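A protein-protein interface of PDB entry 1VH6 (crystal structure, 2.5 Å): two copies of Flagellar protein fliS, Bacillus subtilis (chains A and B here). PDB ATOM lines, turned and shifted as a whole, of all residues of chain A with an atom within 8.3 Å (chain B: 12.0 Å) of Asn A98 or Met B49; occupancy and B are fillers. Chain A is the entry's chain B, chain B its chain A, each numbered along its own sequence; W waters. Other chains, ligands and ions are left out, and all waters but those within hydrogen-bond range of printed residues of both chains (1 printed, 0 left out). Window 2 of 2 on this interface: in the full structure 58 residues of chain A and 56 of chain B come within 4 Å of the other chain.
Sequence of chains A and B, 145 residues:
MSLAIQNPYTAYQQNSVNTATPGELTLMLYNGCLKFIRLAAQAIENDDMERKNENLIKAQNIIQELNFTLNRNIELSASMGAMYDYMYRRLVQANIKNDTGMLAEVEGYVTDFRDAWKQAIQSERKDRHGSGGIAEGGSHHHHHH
The side-chain sulfur of Met B49 sits close to the side-chain amide oxygen of Asn A98 (3.0 Å).
The side-chain amide oxygen (OD1) of Asn A95 lies within hydrogen-bond range of the side-chain amino group (NZ) of Lys B52, 3.0 Å away.
ND2 of Asn A95 lies within hydrogen-bond range of OD1 of Asn B53 (2.9 Å).
The side-chain amide nitrogen (NE2) of Gln B60 is in hydrogen-bond range of the backbone carbonyl oxygen (O) of Leu A91 (3.3 Å).
The side-chain amide nitrogen (NE2) of Gln B60 sits close to the backbone carbonyl oxygen (O) of Leu B56, at 3.2 Å.
Val A92 touches Gln B60.
Asn A95 touches Leu B56.
Ile B44 touches Asn A98 (CG2 to O, 3.6 Å).
Lys B52 touches Asn A98.
CD1 of Ile B44 touches CG2 of Thr A100, at 3.6 Å.
Ile B37 touches Leu A103.
Ala B40 touches Leu A103 (CB to CD1, 3.9 Å).
Leu A103 touches Ala B41 (CD1 to N, 3.7 Å).
Leu A103 touches Ile B44.
CD2 of Leu B56 touches CD2 of Leu A103 (3.7 Å).
No residue of chain B comes within 4 Å of Ala A94.
Of the printed residues of chain B, Asn A98 touches Ile B44 (3.6 Å), Met B49 (3.0 Å) and Lys B52 (2.9 Å).
No residue of chain B comes within 4 Å of Asp A99.
Met A102 touches none of the printed residues of chain B.
Of the printed residues of chain B, Leu A103 touches Ile B37, Ala B40, Ala B41, Ile B44 and Leu B56.
Of the printed residues of chain A, Ala B40 touches Leu A103.
Of the printed residues of chain A, Met B49 touches Asn A98 (3.0 Å).
The nearest residue of chain B that does not touch Asn A98 is Asp B48 (6.7 Å).
Of the 24 printed residues of chain B, 9 touch a printed residue of chain A.
Hydrophobic or aromatic side chains of chain B within 4 Å of the printed part of chain A: Ile B37, Ala B40, Ile B44, Met B49 and Leu B56.
Printed residues of chain A that touch a printed residue of chain B: Leu A91, Val A92, Asn A95, Asn A98, Thr A100 and Leu A103.
Hydrophobic or aromatic side chains of chain A that line the printed part of chain B: Leu A91, Val A92 and Leu A103.
No position is printed for both chains.
Water W1 lies within hydrogen-bond range of the side-chain amide nitrogen of Asn A95 (2.7 Å) and the side-chain amide oxygen of Gln B60 (3.4 Å).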
ATOM      1  N   LEU A  91      18.592 -14.805   2.077  1.00  0.00           N
ATOM      2  CA  LEU A  91      19.296 -15.335   3.246  1.00  0.00           C
ATOM      3  C   LEU A  91      19.657 -14.199   4.204  1.00  0.00           C
ATOM      4  O   LEU A  91      19.713 -14.383   5.425  1.00  0.00           O
ATOM      5  CB  LEU A  91      20.567 -16.074   2.819  1.00  0.00           C
ATOM      6  CG  LEU A  91      20.337 -17.426   2.150  1.00  0.00           C
ATOM      7  CD1 LEU A  91      21.667 -18.122   1.854  1.00  0.00           C
ATOM      8  CD2 LEU A  91      19.505 -18.278   3.075  1.00  0.00           C
ATOM      9  N   VAL A  92      19.900 -13.022   3.637  1.00  0.00           N
ATOM     10  CA  VAL A  92      20.228 -11.855   4.430  1.00  0.00           C
ATOM     11  C   VAL A  92      18.968 -11.391   5.132  1.00  0.00           C
ATOM     12  O   VAL A  92      19.006 -10.977   6.292  1.00  0.00           O
ATOM     13  CB  VAL A  92      20.780 -10.722   3.542  1.00  0.00           C
ATOM     14  CG1 VAL A  92      20.846  -9.421   4.320  1.00  0.00           C
ATOM     15  CG2 VAL A  92      22.164 -11.102   3.042  1.00  0.00           C
ATOM     16  N   GLN A  93      17.845 -11.485   4.427  1.00  0.00           N
ATOM     17  CA  GLN A  93      16.560 -11.069   4.969  1.00  0.00           C
ATOM     18  C   GLN A  93      16.036 -12.090   5.970  1.00  0.00           C
ATOM     19  O   GLN A  93      15.261 -11.749   6.863  1.00  0.00           O
ATOM     20  CB  GLN A  93      15.550 -10.880   3.839  1.00  0.00           C
ATOM     21  CG  GLN A  93      14.401  -9.942   4.177  1.00  0.00           C
ATOM     22  CD  GLN A  93      14.882  -8.594   4.713  1.00  0.00           C
ATOM     23  OE1 GLN A  93      15.960  -8.114   4.341  1.00  0.00           O
ATOM     24  NE2 GLN A  93      14.076  -7.972   5.577  1.00  0.00           N
ATOM     25  N   ALA A  94      16.453 -13.343   5.826  1.00  0.00           N
ATOM     26  CA  ALA A  94      16.019 -14.390   6.742  1.00  0.00           C
ATOM     27  C   ALA A  94      16.874 -14.333   8.009  1.00  0.00           C
ATOM     28  O   ALA A  94      16.457 -14.766   9.088  1.00  0.00           O
ATOM     29  CB  ALA A  94      16.153 -15.757   6.083  1.00  0.00           C
ATOM     30  N   ASN A  95      18.076 -13.787   7.866  1.00  0.00           N
ATOM     31  CA  ASN A  95      18.992 -13.678   8.984  1.00  0.00           C
ATOM     32  C   ASN A  95      18.653 -12.501   9.882  1.00  0.00           C
ATOM     33  O   ASN A  95      19.049 -12.466  11.041  1.00  0.00           O
ATOM     34  CB  ASN A  95      20.422 -13.536   8.469  1.00  0.00           C
ATOM     35  CG  ASN A  95      21.440 -13.575   9.582  1.00  0.00           C
ATOM     36  OD1 ASN A  95      21.226 -14.231  10.599  1.00  0.00           O
ATOM     37  ND2 ASN A  95      22.564 -12.891   9.389  1.00  0.00           N
ATOM     38  N   ILE A  96      17.917 -11.537   9.340  1.00  0.00           N
ATOM     39  CA  ILE A  96      17.535 -10.349  10.088  1.00  0.00           C
ATOM     40  C   ILE A  96      16.181 -10.525  10.765  1.00  0.00           C
ATOM     41  O   ILE A  96      15.910  -9.928  11.813  1.00  0.00           O
ATOM     42  CB  ILE A  96      17.485  -9.121   9.153  1.00  0.00           C
ATOM     43  CG1 ILE A  96      18.910  -8.672   8.820  1.00  0.00           C
ATOM     44  CG2 ILE A  96      16.681  -7.994   9.792  1.00  0.00           C
ATOM     45  CD1 ILE A  96      18.974  -7.553   7.804  1.00  0.00           C
ATOM     46  N   LYS A  97      15.334 -11.353  10.166  1.00  0.00           N
ATOM     47  CA  LYS A  97      14.012 -11.588  10.716  1.00  0.00           C
ATOM     48  C   LYS A  97      13.824 -12.967  11.346  1.00  0.00           C
ATOM     49  O   LYS A  97      12.738 -13.288  11.827  1.00  0.00           O
ATOM     50  CB  LYS A  97      12.957 -11.344   9.636  1.00  0.00           C
ATOM     51  CG  LYS A  97      12.851  -9.876   9.255  1.00  0.00           C
ATOM     52  CD  LYS A  97      11.815  -9.622   8.168  1.00  0.00           C
ATOM     53  CE  LYS A  97      11.601  -8.123   7.987  1.00  0.00           C
ATOM     54  NZ  LYS A  97      10.654  -7.795   6.883  1.00  0.00           N
ATOM     55  N   ASN A  98      14.880 -13.779  11.362  1.00  0.00           N
ATOM     56  CA  ASN A  98      14.785 -15.109  11.959  1.00  0.00           C
ATOM     57  C   ASN A  98      13.571 -15.828  11.376  1.00  0.00           C
ATOM     58  O   ASN A  98      12.760 -16.425  12.093  1.00  0.00           O
ATOM     59  CB  ASN A  98      14.662 -14.974  13.478  1.00  0.00           C
ATOM     60  CG  ASN A  98      15.903 -14.360  14.102  1.00  0.00           C
ATOM     61  OD1 ASN A  98      16.943 -15.002  14.184  1.00  0.00           O
ATOM     62  ND2 ASN A  98      15.804 -13.104  14.525  1.00  0.00           N
ATOM     63  N   ASP A  99      13.476 -15.763  10.051  1.00  0.00           N
ATOM     64  CA  ASP A  99      12.382 -16.358   9.313  1.00  0.00           C
ATOM     65  C   ASP A  99      12.744 -17.711   8.694  1.00  0.00           C
ATOM     66  O   ASP A  99      13.177 -17.783   7.543  1.00  0.00           O
ATOM     67  CB  ASP A  99      11.937 -15.380   8.227  1.00  0.00           C
ATOM     68  CG  ASP A  99      10.719 -15.862   7.465  1.00  0.00           C
ATOM     69  OD1 ASP A  99      10.334 -15.173   6.492  1.00  0.00           O
ATOM     70  OD2 ASP A  99      10.145 -16.915   7.835  1.00  0.00           O
ATOM     71  N   THR A 100      12.572 -18.785   9.457  1.00  0.00           N
ATOM     72  CA  THR A 100      12.871 -20.113   8.938  1.00  0.00           C
ATOM     73  C   THR A 100      12.066 -20.335   7.658  1.00  0.00           C
ATOM     74  O   THR A 100      12.382 -21.216   6.856  1.00  0.00           O
ATOM     75  CB  THR A 100      12.502 -21.206   9.947  1.00  0.00           C
ATOM     76  OG1 THR A 100      11.124 -21.079  10.301  1.00  0.00           O
ATOM     77  CG2 THR A 100      13.353 -21.081  11.197  1.00  0.00           C
ATOM     78  N   GLY A 101      11.026 -19.527   7.474  1.00  0.00           N
ATOM     79  CA  GLY A 101      10.197 -19.640   6.291  1.00  0.00           C
ATOM     80  C   GLY A 101      10.983 -19.338   5.028  1.00  0.00           C
ATOM     81  O   GLY A 101      10.884 -20.063   4.036  1.00  0.00           O
ATOM     82  N   MET A 102      11.765 -18.264   5.068  1.00  0.00           N
ATOM     83  CA  MET A 102      12.577 -17.855   3.933  1.00  0.00           C
ATOM     84  C   MET A 102      13.715 -18.828   3.678  1.00  0.00           C
ATOM     85  O   MET A 102      14.174 -18.972   2.540  1.00  0.00           O
ATOM     86  CB  MET A 102      13.141 -16.462   4.165  1.00  0.00           C
ATOM     87  CG  MET A 102      12.106 -15.372   4.099  1.00  0.00           C
ATOM     88  SD  MET A 102      12.927 -13.639   4.203  1.00  0.00           S
ATOM     89  CE  MET A 102      11.839 -12.900   5.627  1.00  0.00           C
ATOM     90  N   LEU A 103      14.176 -19.491   4.736  1.00  0.00           N
ATOM     91  CA  LEU A 103      15.246 -20.466   4.587  1.00  0.00           C
ATOM     92  C   LEU A 103      14.679 -21.682   3.863  1.00  0.00           C
ATOM     93  O   LEU A 103      15.388 -22.378   3.138  1.00  0.00           O
ATOM     94  CB  LEU A 103      15.791 -20.887   5.954  1.00  0.00           C
ATOM     95  CG  LEU A 103      16.364 -19.781   6.843  1.00  0.00           C
ATOM     96  CD1 LEU A 103      16.987 -20.402   8.075  1.00  0.00           C
ATOM     97  CD2 LEU A 103      17.394 -18.972   6.071  1.00  0.00           C
ATOM     98  N   PHE B  36      24.556 -25.598   5.686  1.00  0.00           N
ATOM     99  CA  PHE B  36      24.542 -24.364   6.460  1.00  0.00           C
ATOM    100  C   PHE B  36      23.156 -23.742   6.560  1.00  0.00           C
ATOM    101  O   PHE B  36      22.821 -23.139   7.581  1.00  0.00           O
ATOM    102  CB  PHE B  36      25.548 -23.382   5.864  1.00  0.00           C
ATOM    103  CG  PHE B  36      26.952 -23.919   5.841  1.00  0.00           C
ATOM    104  CD1 PHE B  36      27.795 -23.666   4.764  1.00  0.00           C
ATOM    105  CD2 PHE B  36      27.424 -24.706   6.894  1.00  0.00           C
ATOM    106  CE1 PHE B  36      29.084 -24.189   4.727  1.00  0.00           C
ATOM    107  CE2 PHE B  36      28.715 -25.233   6.866  1.00  0.00           C
ATOM    108  CZ  PHE B  36      29.547 -24.972   5.776  1.00  0.00           C
ATOM    109  N   ILE B  37      22.352 -23.881   5.509  1.00  0.00           N
ATOM    110  CA  ILE B  37      20.993 -23.352   5.532  1.00  0.00           C
ATOM    111  C   ILE B  37      20.185 -24.175   6.539  1.00  0.00           C
ATOM    112  O   ILE B  37      19.387 -23.634   7.306  1.00  0.00           O
ATOM    113  CB  ILE B  37      20.298 -23.473   4.156  1.00  0.00           C
ATOM    114  CG1 ILE B  37      20.917 -22.489   3.160  1.00  0.00           C
ATOM    115  CG2 ILE B  37      18.803 -23.239   4.304  1.00  0.00           C
ATOM    116  CD1 ILE B  37      20.204 -22.452   1.826  1.00  0.00           C
ATOM    117  N   ARG B  38      20.401 -25.485   6.535  1.00  0.00           N
ATOM    118  CA  ARG B  38      19.677 -26.365   7.438  1.00  0.00           C
ATOM    119  C   ARG B  38      20.056 -26.173   8.908  1.00  0.00           C
ATOM    120  O   ARG B  38      19.194 -26.238   9.787  1.00  0.00           O
ATOM    121  CB  ARG B  38      19.891 -27.820   7.022  1.00  0.00           C
ATOM    122  CG  ARG B  38      19.179 -28.186   5.724  1.00  0.00           C
ATOM    123  CD  ARG B  38      19.622 -29.547   5.238  1.00  0.00           C
ATOM    124  NE  ARG B  38      19.079 -29.857   3.923  1.00  0.00           N
ATOM    125  CZ  ARG B  38      19.519 -30.852   3.160  1.00  0.00           C
ATOM    126  NH1 ARG B  38      20.511 -31.622   3.589  1.00  0.00           N
ATOM    127  NH2 ARG B  38      18.968 -31.074   1.975  1.00  0.00           N
ATOM    128  N   LEU B  39      21.340 -25.941   9.170  1.00  0.00           N
ATOM    129  CA  LEU B  39      21.814 -25.719  10.531  1.00  0.00           C
ATOM    130  C   LEU B  39      21.291 -24.383  11.050  1.00  0.00           C
ATOM    131  O   LEU B  39      21.141 -24.187  12.253  1.00  0.00           O
ATOM    132  CB  LEU B  39      23.350 -25.720  10.567  1.00  0.00           C
ATOM    133  CG  LEU B  39      24.035 -27.084  10.439  1.00  0.00           C
ATOM    134  CD1 LEU B  39      25.545 -26.901  10.392  1.00  0.00           C
ATOM    135  CD2 LEU B  39      23.629 -27.965  11.616  1.00  0.00           C
ATOM    136  N   ALA B  40      21.024 -23.462  10.130  1.00  0.00           N
ATOM    137  CA  ALA B  40      20.520 -22.143  10.492  1.00  0.00           C
ATOM    138  C   ALA B  40      19.062 -22.257  10.924  1.00  0.00           C
ATOM    139  O   ALA B  40      18.621 -21.561  11.832  1.00  0.00           O
ATOM    140  CB  ALA B  40      20.649 -21.186   9.309  1.00  0.00           C
ATOM    141  N   ALA B  41      18.314 -23.138  10.268  1.00  0.00           N
ATOM    142  CA  ALA B  41      16.914 -23.336  10.618  1.00  0.00           C
ATOM    143  C   ALA B  41      16.867 -23.941  12.023  1.00  0.00           C
ATOM    144  O   ALA B  41      16.004 -23.598  12.830  1.00  0.00           O
ATOM    145  CB  ALA B  41      16.237 -24.268   9.601  1.00  0.00           C
ATOM    146  N   GLN B  42      17.806 -24.842  12.302  1.00  0.00           N
ATOM    147  CA  GLN B  42      17.908 -25.487  13.610  1.00  0.00           C
ATOM    148  C   GLN B  42      18.229 -24.460  14.694  1.00  0.00           C
ATOM    149  O   GLN B  42      17.644 -24.474  15.779  1.00  0.00           O
ATOM    150  CB  GLN B  42      19.022 -26.534  13.612  1.00  0.00           C
ATOM    151  CG  GLN B  42      18.790 -27.748  12.739  1.00  0.00           C
ATOM    152  CD  GLN B  42      19.989 -28.697  12.761  1.00  0.00           C
ATOM    153  OE1 GLN B  42      20.607 -28.917  13.818  1.00  0.00           O
ATOM    154  NE2 GLN B  42      20.319 -29.269  11.597  1.00  0.00           N
ATOM    155  N   ALA B  43      19.172 -23.575  14.397  1.00  0.00           N
ATOM    156  CA  ALA B  43      19.576 -22.558  15.351  1.00  0.00           C
ATOM    157  C   ALA B  43      18.446 -21.602  15.715  1.00  0.00           C
ATOM    158  O   ALA B  43      18.257 -21.296  16.893  1.00  0.00           O
ATOM    159  CB  ALA B  43      20.776 -21.778  14.810  1.00  0.00           C
ATOM    160  N   ILE B  44      17.695 -21.137  14.719  1.00  0.00           N
ATOM    161  CA  ILE B  44      16.593 -20.205  14.972  1.00  0.00           C
ATOM    162  C   ILE B  44      15.558 -20.791  15.932  1.00  0.00           C
ATOM    163  O   ILE B  44      15.056 -20.095  16.826  1.00  0.00           O
ATOM    164  CB  ILE B  44      15.863 -19.798  13.671  1.00  0.00           C
ATOM    165  CG1 ILE B  44      16.865 -19.242  12.655  1.00  0.00           C
ATOM    166  CG2 ILE B  44      14.814 -18.733  13.983  1.00  0.00           C
ATOM    167  CD1 ILE B  44      16.272 -18.949  11.294  1.00  0.00           C
ATOM    168  N   GLU B  45      15.245 -22.071  15.749  1.00  0.00           N
ATOM    169  CA  GLU B  45      14.278 -22.742  16.604  1.00  0.00           C
ATOM    170  C   GLU B  45      14.790 -22.869  18.031  1.00  0.00           C
ATOM    171  O   GLU B  45      14.004 -22.826  18.969  1.00  0.00           O
ATOM    172  CB  GLU B  45      13.943 -24.123  16.039  1.00  0.00           C
ATOM    173  CG  GLU B  45      13.428 -24.052  14.613  1.00  0.00           C
ATOM    174  CD  GLU B  45      12.761 -25.336  14.153  1.00  0.00           C
ATOM    175  OE1 GLU B  45      12.365 -25.398  12.963  1.00  0.00           O
ATOM    176  OE2 GLU B  45      12.626 -26.274  14.976  1.00  0.00           O
ATOM    177  N   ASN B  46      16.103 -23.022  18.195  1.00  0.00           N
ATOM    178  CA  ASN B  46      16.702 -23.135  19.523  1.00  0.00           C
ATOM    179  C   ASN B  46      17.151 -21.767  20.018  1.00  0.00           C
ATOM    180  O   ASN B  46      17.954 -21.675  20.952  1.00  0.00           O
ATOM    181  CB  ASN B  46      17.922 -24.051  19.495  1.00  0.00           C
ATOM    182  CG  ASN B  46      17.623 -25.408  18.902  1.00  0.00           C
ATOM    183  OD1 ASN B  46      16.471 -25.838  18.853  1.00  0.00           O
ATOM    184  ND2 ASN B  46      18.664 -26.100  18.461  1.00  0.00           N
ATOM    185  N   ASP B  47      16.627 -20.710  19.395  1.00  0.00           N
ATOM    186  CA  ASP B  47      16.996 -19.339  19.742  1.00  0.00           C
ATOM    187  C   ASP B  47      18.508 -19.224  19.862  1.00  0.00           C
ATOM    188  O   ASP B  47      19.022 -18.562  20.765  1.00  0.00           O
ATOM    189  CB  ASP B  47      16.350 -18.897  21.057  1.00  0.00           C
ATOM    190  CG  ASP B  47      14.891 -18.519  20.894  1.00  0.00           C
ATOM    191  OD1 ASP B  47      14.530 -17.965  19.833  1.00  0.00           O
ATOM    192  OD2 ASP B  47      14.107 -18.762  21.837  1.00  0.00           O
ATOM    193  N   ASP B  48      19.209 -19.887  18.949  1.00  0.00           N
ATOM    194  CA  ASP B  48      20.666 -19.873  18.924  1.00  0.00           C
ATOM    195  C   ASP B  48      21.115 -18.863  17.869  1.00  0.00           C
ATOM    196  O   ASP B  48      21.440 -19.240  16.743  1.00  0.00           O
ATOM    197  CB  ASP B  48      21.176 -21.262  18.555  1.00  0.00           C
ATOM    198  CG  ASP B  48      22.674 -21.402  18.712  1.00  0.00           C
ATOM    199  OD1 ASP B  48      23.392 -20.380  18.695  1.00  0.00           O
ATOM    200  OD2 ASP B  48      23.132 -22.555  18.840  1.00  0.00           O
ATOM    201  N   MET B  49      21.126 -17.582  18.229  1.00  0.00           N
ATOM    202  CA  MET B  49      21.513 -16.536  17.288  1.00  0.00           C
ATOM    203  C   MET B  49      22.973 -16.623  16.858  1.00  0.00           C
ATOM    204  O   MET B  49      23.339 -16.186  15.764  1.00  0.00           O
ATOM    205  CB  MET B  49      21.226 -15.161  17.894  1.00  0.00           C
ATOM    206  CG  MET B  49      19.761 -14.938  18.234  1.00  0.00           C
ATOM    207  SD  MET B  49      18.547 -15.159  16.719  1.00  0.00           S
ATOM    208  CE  MET B  49      18.371 -13.282  16.236  1.00  0.00           C
ATOM    209  N   GLU B  50      23.803 -17.197  17.718  1.00  0.00           N
ATOM    210  CA  GLU B  50      25.222 -17.338  17.434  1.00  0.00           C
ATOM    211  C   GLU B  50      25.439 -18.157  16.171  1.00  0.00           C
ATOM    212  O   GLU B  50      25.979 -17.664  15.182  1.00  0.00           O
ATOM    213  CB  GLU B  50      25.920 -18.041  18.605  1.00  0.00           C
ATOM    214  CG  GLU B  50      25.612 -17.440  19.971  1.00  0.00           C
ATOM    215  CD  GLU B  50      26.315 -16.113  20.189  1.00  0.00           C
ATOM    216  OE1 GLU B  50      26.029 -15.447  21.210  1.00  0.00           O
ATOM    217  OE2 GLU B  50      27.159 -15.746  19.337  1.00  0.00           O
ATOM    218  N   ARG B  51      25.015 -19.416  16.228  1.00  0.00           N
ATOM    219  CA  ARG B  51      25.164 -20.357  15.130  1.00  0.00           C
ATOM    220  C   ARG B  51      24.321 -20.019  13.906  1.00  0.00           C
ATOM    221  O   ARG B  51      24.665 -20.400  12.786  1.00  0.00           O
ATOM    222  CB  ARG B  51      24.843 -21.769  15.622  1.00  0.00           C
ATOM    223  CG  ARG B  51      25.811 -22.266  16.687  1.00  0.00           C
ATOM    224  CD  ARG B  51      25.511 -23.693  17.125  1.00  0.00           C
ATOM    225  NE  ARG B  51      26.501 -24.179  18.083  1.00  0.00           N
ATOM    226  CZ  ARG B  51      26.760 -23.597  19.253  1.00  0.00           C
ATOM    227  NH1 ARG B  51      26.099 -22.504  19.616  1.00  0.00           N
ATOM    228  NH2 ARG B  51      27.688 -24.103  20.061  1.00  0.00           N
ATOM    229  N   LYS B  52      23.218 -19.309  14.115  1.00  0.00           N
ATOM    230  CA  LYS B  52      22.364 -18.916  13.001  1.00  0.00           C
ATOM    231  C   LYS B  52      23.141 -17.999  12.063  1.00  0.00           C
ATOM    232  O   LYS B  52      23.152 -18.189  10.848  1.00  0.00           O
ATOM    233  CB  LYS B  52      21.134 -18.155  13.501  1.00  0.00           C
ATOM    234  CG  LYS B  52      20.229 -17.655  12.381  1.00  0.00           C
ATOM    235  CD  LYS B  52      19.120 -16.764  12.904  1.00  0.00           C
ATOM    236  CE  LYS B  52      19.537 -15.306  12.888  1.00  0.00           C
ATOM    237  NZ  LYS B  52      20.886 -15.124  13.453  1.00  0.00           N
ATOM    238  N   ASN B  53      23.782 -16.996  12.647  1.00  0.00           N
ATOM    239  CA  ASN B  53      24.548 -16.022  11.890  1.00  0.00           C
ATOM    240  C   ASN B  53      25.717 -16.707  11.197  1.00  0.00           C
ATOM    241  O   ASN B  53      25.909 -16.569   9.987  1.00  0.00           O
ATOM    242  CB  ASN B  53      25.043 -14.918  12.833  1.00  0.00           C
ATOM    243  CG  ASN B  53      25.512 -13.683  12.095  1.00  0.00           C
ATOM    244  OD1 ASN B  53      24.775 -13.097  11.303  1.00  0.00           O
ATOM    245  ND2 ASN B  53      26.746 -13.276  12.354  1.00  0.00           N
ATOM    246  N   GLU B  54      26.488 -17.461  11.965  1.00  0.00           N
ATOM    247  CA  GLU B  54      27.635 -18.170  11.421  1.00  0.00           C
ATOM    248  C   GLU B  54      27.231 -18.925  10.142  1.00  0.00           C
ATOM    249  O   GLU B  54      27.730 -18.635   9.050  1.00  0.00           O
ATOM    250  CB  GLU B  54      28.177 -19.141  12.482  1.00  0.00           C
ATOM    251  CG  GLU B  54      29.519 -19.769  12.159  1.00  0.00           C
ATOM    252  N   ASN B  55      26.304 -19.871  10.288  1.00  0.00           N
ATOM    253  CA  ASN B  55      25.819 -20.690   9.184  1.00  0.00           C
ATOM    254  C   ASN B  55      25.184 -19.913   8.044  1.00  0.00           C
ATOM    255  O   ASN B  55      25.297 -20.313   6.889  1.00  0.00           O
ATOM    256  CB  ASN B  55      24.825 -21.719   9.711  1.00  0.00           C
ATOM    257  CG  ASN B  55      25.495 -22.795  10.536  1.00  0.00           C
ATOM    258  OD1 ASN B  55      26.142 -23.687   9.993  1.00  0.00           O
ATOM    259  ND2 ASN B  55      25.358 -22.709  11.857  1.00  0.00           N
ATOM    260  N   LEU B  56      24.509 -18.811   8.348  1.00  0.00           N
ATOM    261  CA  LEU B  56      23.889 -18.024   7.286  1.00  0.00           C
ATOM    262  C   LEU B  56      24.916 -17.249   6.477  1.00  0.00           C
ATOM    263  O   LEU B  56      24.743 -17.036   5.282  1.00  0.00           O
ATOM    264  CB  LEU B  56      22.846 -17.069   7.860  1.00  0.00           C
ATOM    265  CG  LEU B  56      21.512 -17.746   8.154  1.00  0.00           C
ATOM    266  CD1 LEU B  56      20.524 -16.750   8.720  1.00  0.00           C
ATOM    267  CD2 LEU B  56      21.000 -18.360   6.862  1.00  0.00           C
ATOM    268  N   ILE B  57      25.990 -16.822   7.123  1.00  0.00           N
ATOM    269  CA  ILE B  57      27.026 -16.103   6.408  1.00  0.00           C
ATOM    270  C   ILE B  57      27.764 -17.082   5.494  1.00  0.00           C
ATOM    271  O   ILE B  57      28.079 -16.746   4.352  1.00  0.00           O
ATOM    272  CB  ILE B  57      28.015 -15.422   7.386  1.00  0.00           C
ATOM    273  CG1 ILE B  57      27.377 -14.150   7.948  1.00  0.00           C
ATOM    274  CG2 ILE B  57      29.318 -15.089   6.678  1.00  0.00           C
ATOM    275  CD1 ILE B  57      28.208 -13.465   9.019  1.00  0.00           C
ATOM    276  N   LYS B  58      28.019 -18.293   5.990  1.00  0.00           N
ATOM    277  CA  LYS B  58      28.712 -19.318   5.206  1.00  0.00           C
ATOM    278  C   LYS B  58      27.924 -19.667   3.950  1.00  0.00           C
ATOM    279  O   LYS B  58      28.489 -19.785   2.864  1.00  0.00           O
ATOM    280  CB  LYS B  58      28.895 -20.597   6.015  1.00  0.00           C
ATOM    281  CG  LYS B  58      29.907 -20.549   7.132  1.00  0.00           C
ATOM    282  CD  LYS B  58      29.934 -21.921   7.782  1.00  0.00           C
ATOM    283  CE  LYS B  58      30.907 -22.020   8.931  1.00  0.00           C
ATOM    284  NZ  LYS B  58      31.052 -23.453   9.342  1.00  0.00           N
ATOM    285  N   GLN B  60      25.811 -17.788   2.565  1.00  0.00           N
ATOM    286  CA  GLN B  60      25.849 -16.582   1.750  1.00  0.00           C
ATOM    287  C   GLN B  60      27.167 -16.489   0.981  1.00  0.00           C
ATOM    288  O   GLN B  60      27.180 -16.104  -0.193  1.00  0.00           O
ATOM    289  CB  GLN B  60      25.683 -15.348   2.632  1.00  0.00           C
ATOM    290  CG  GLN B  60      24.221 -14.968   2.903  1.00  0.00           C
ATOM    291  CD  GLN B  60      24.066 -14.129   4.152  1.00  0.00           C
ATOM    292  OE1 GLN B  60      24.903 -13.284   4.451  1.00  0.00           O
ATOM    293  NE2 GLN B  60      22.987 -14.353   4.880  1.00  0.00           N
HETATM  294  O   HOH W   1      23.579 -11.748   7.165  1.00  0.00           O
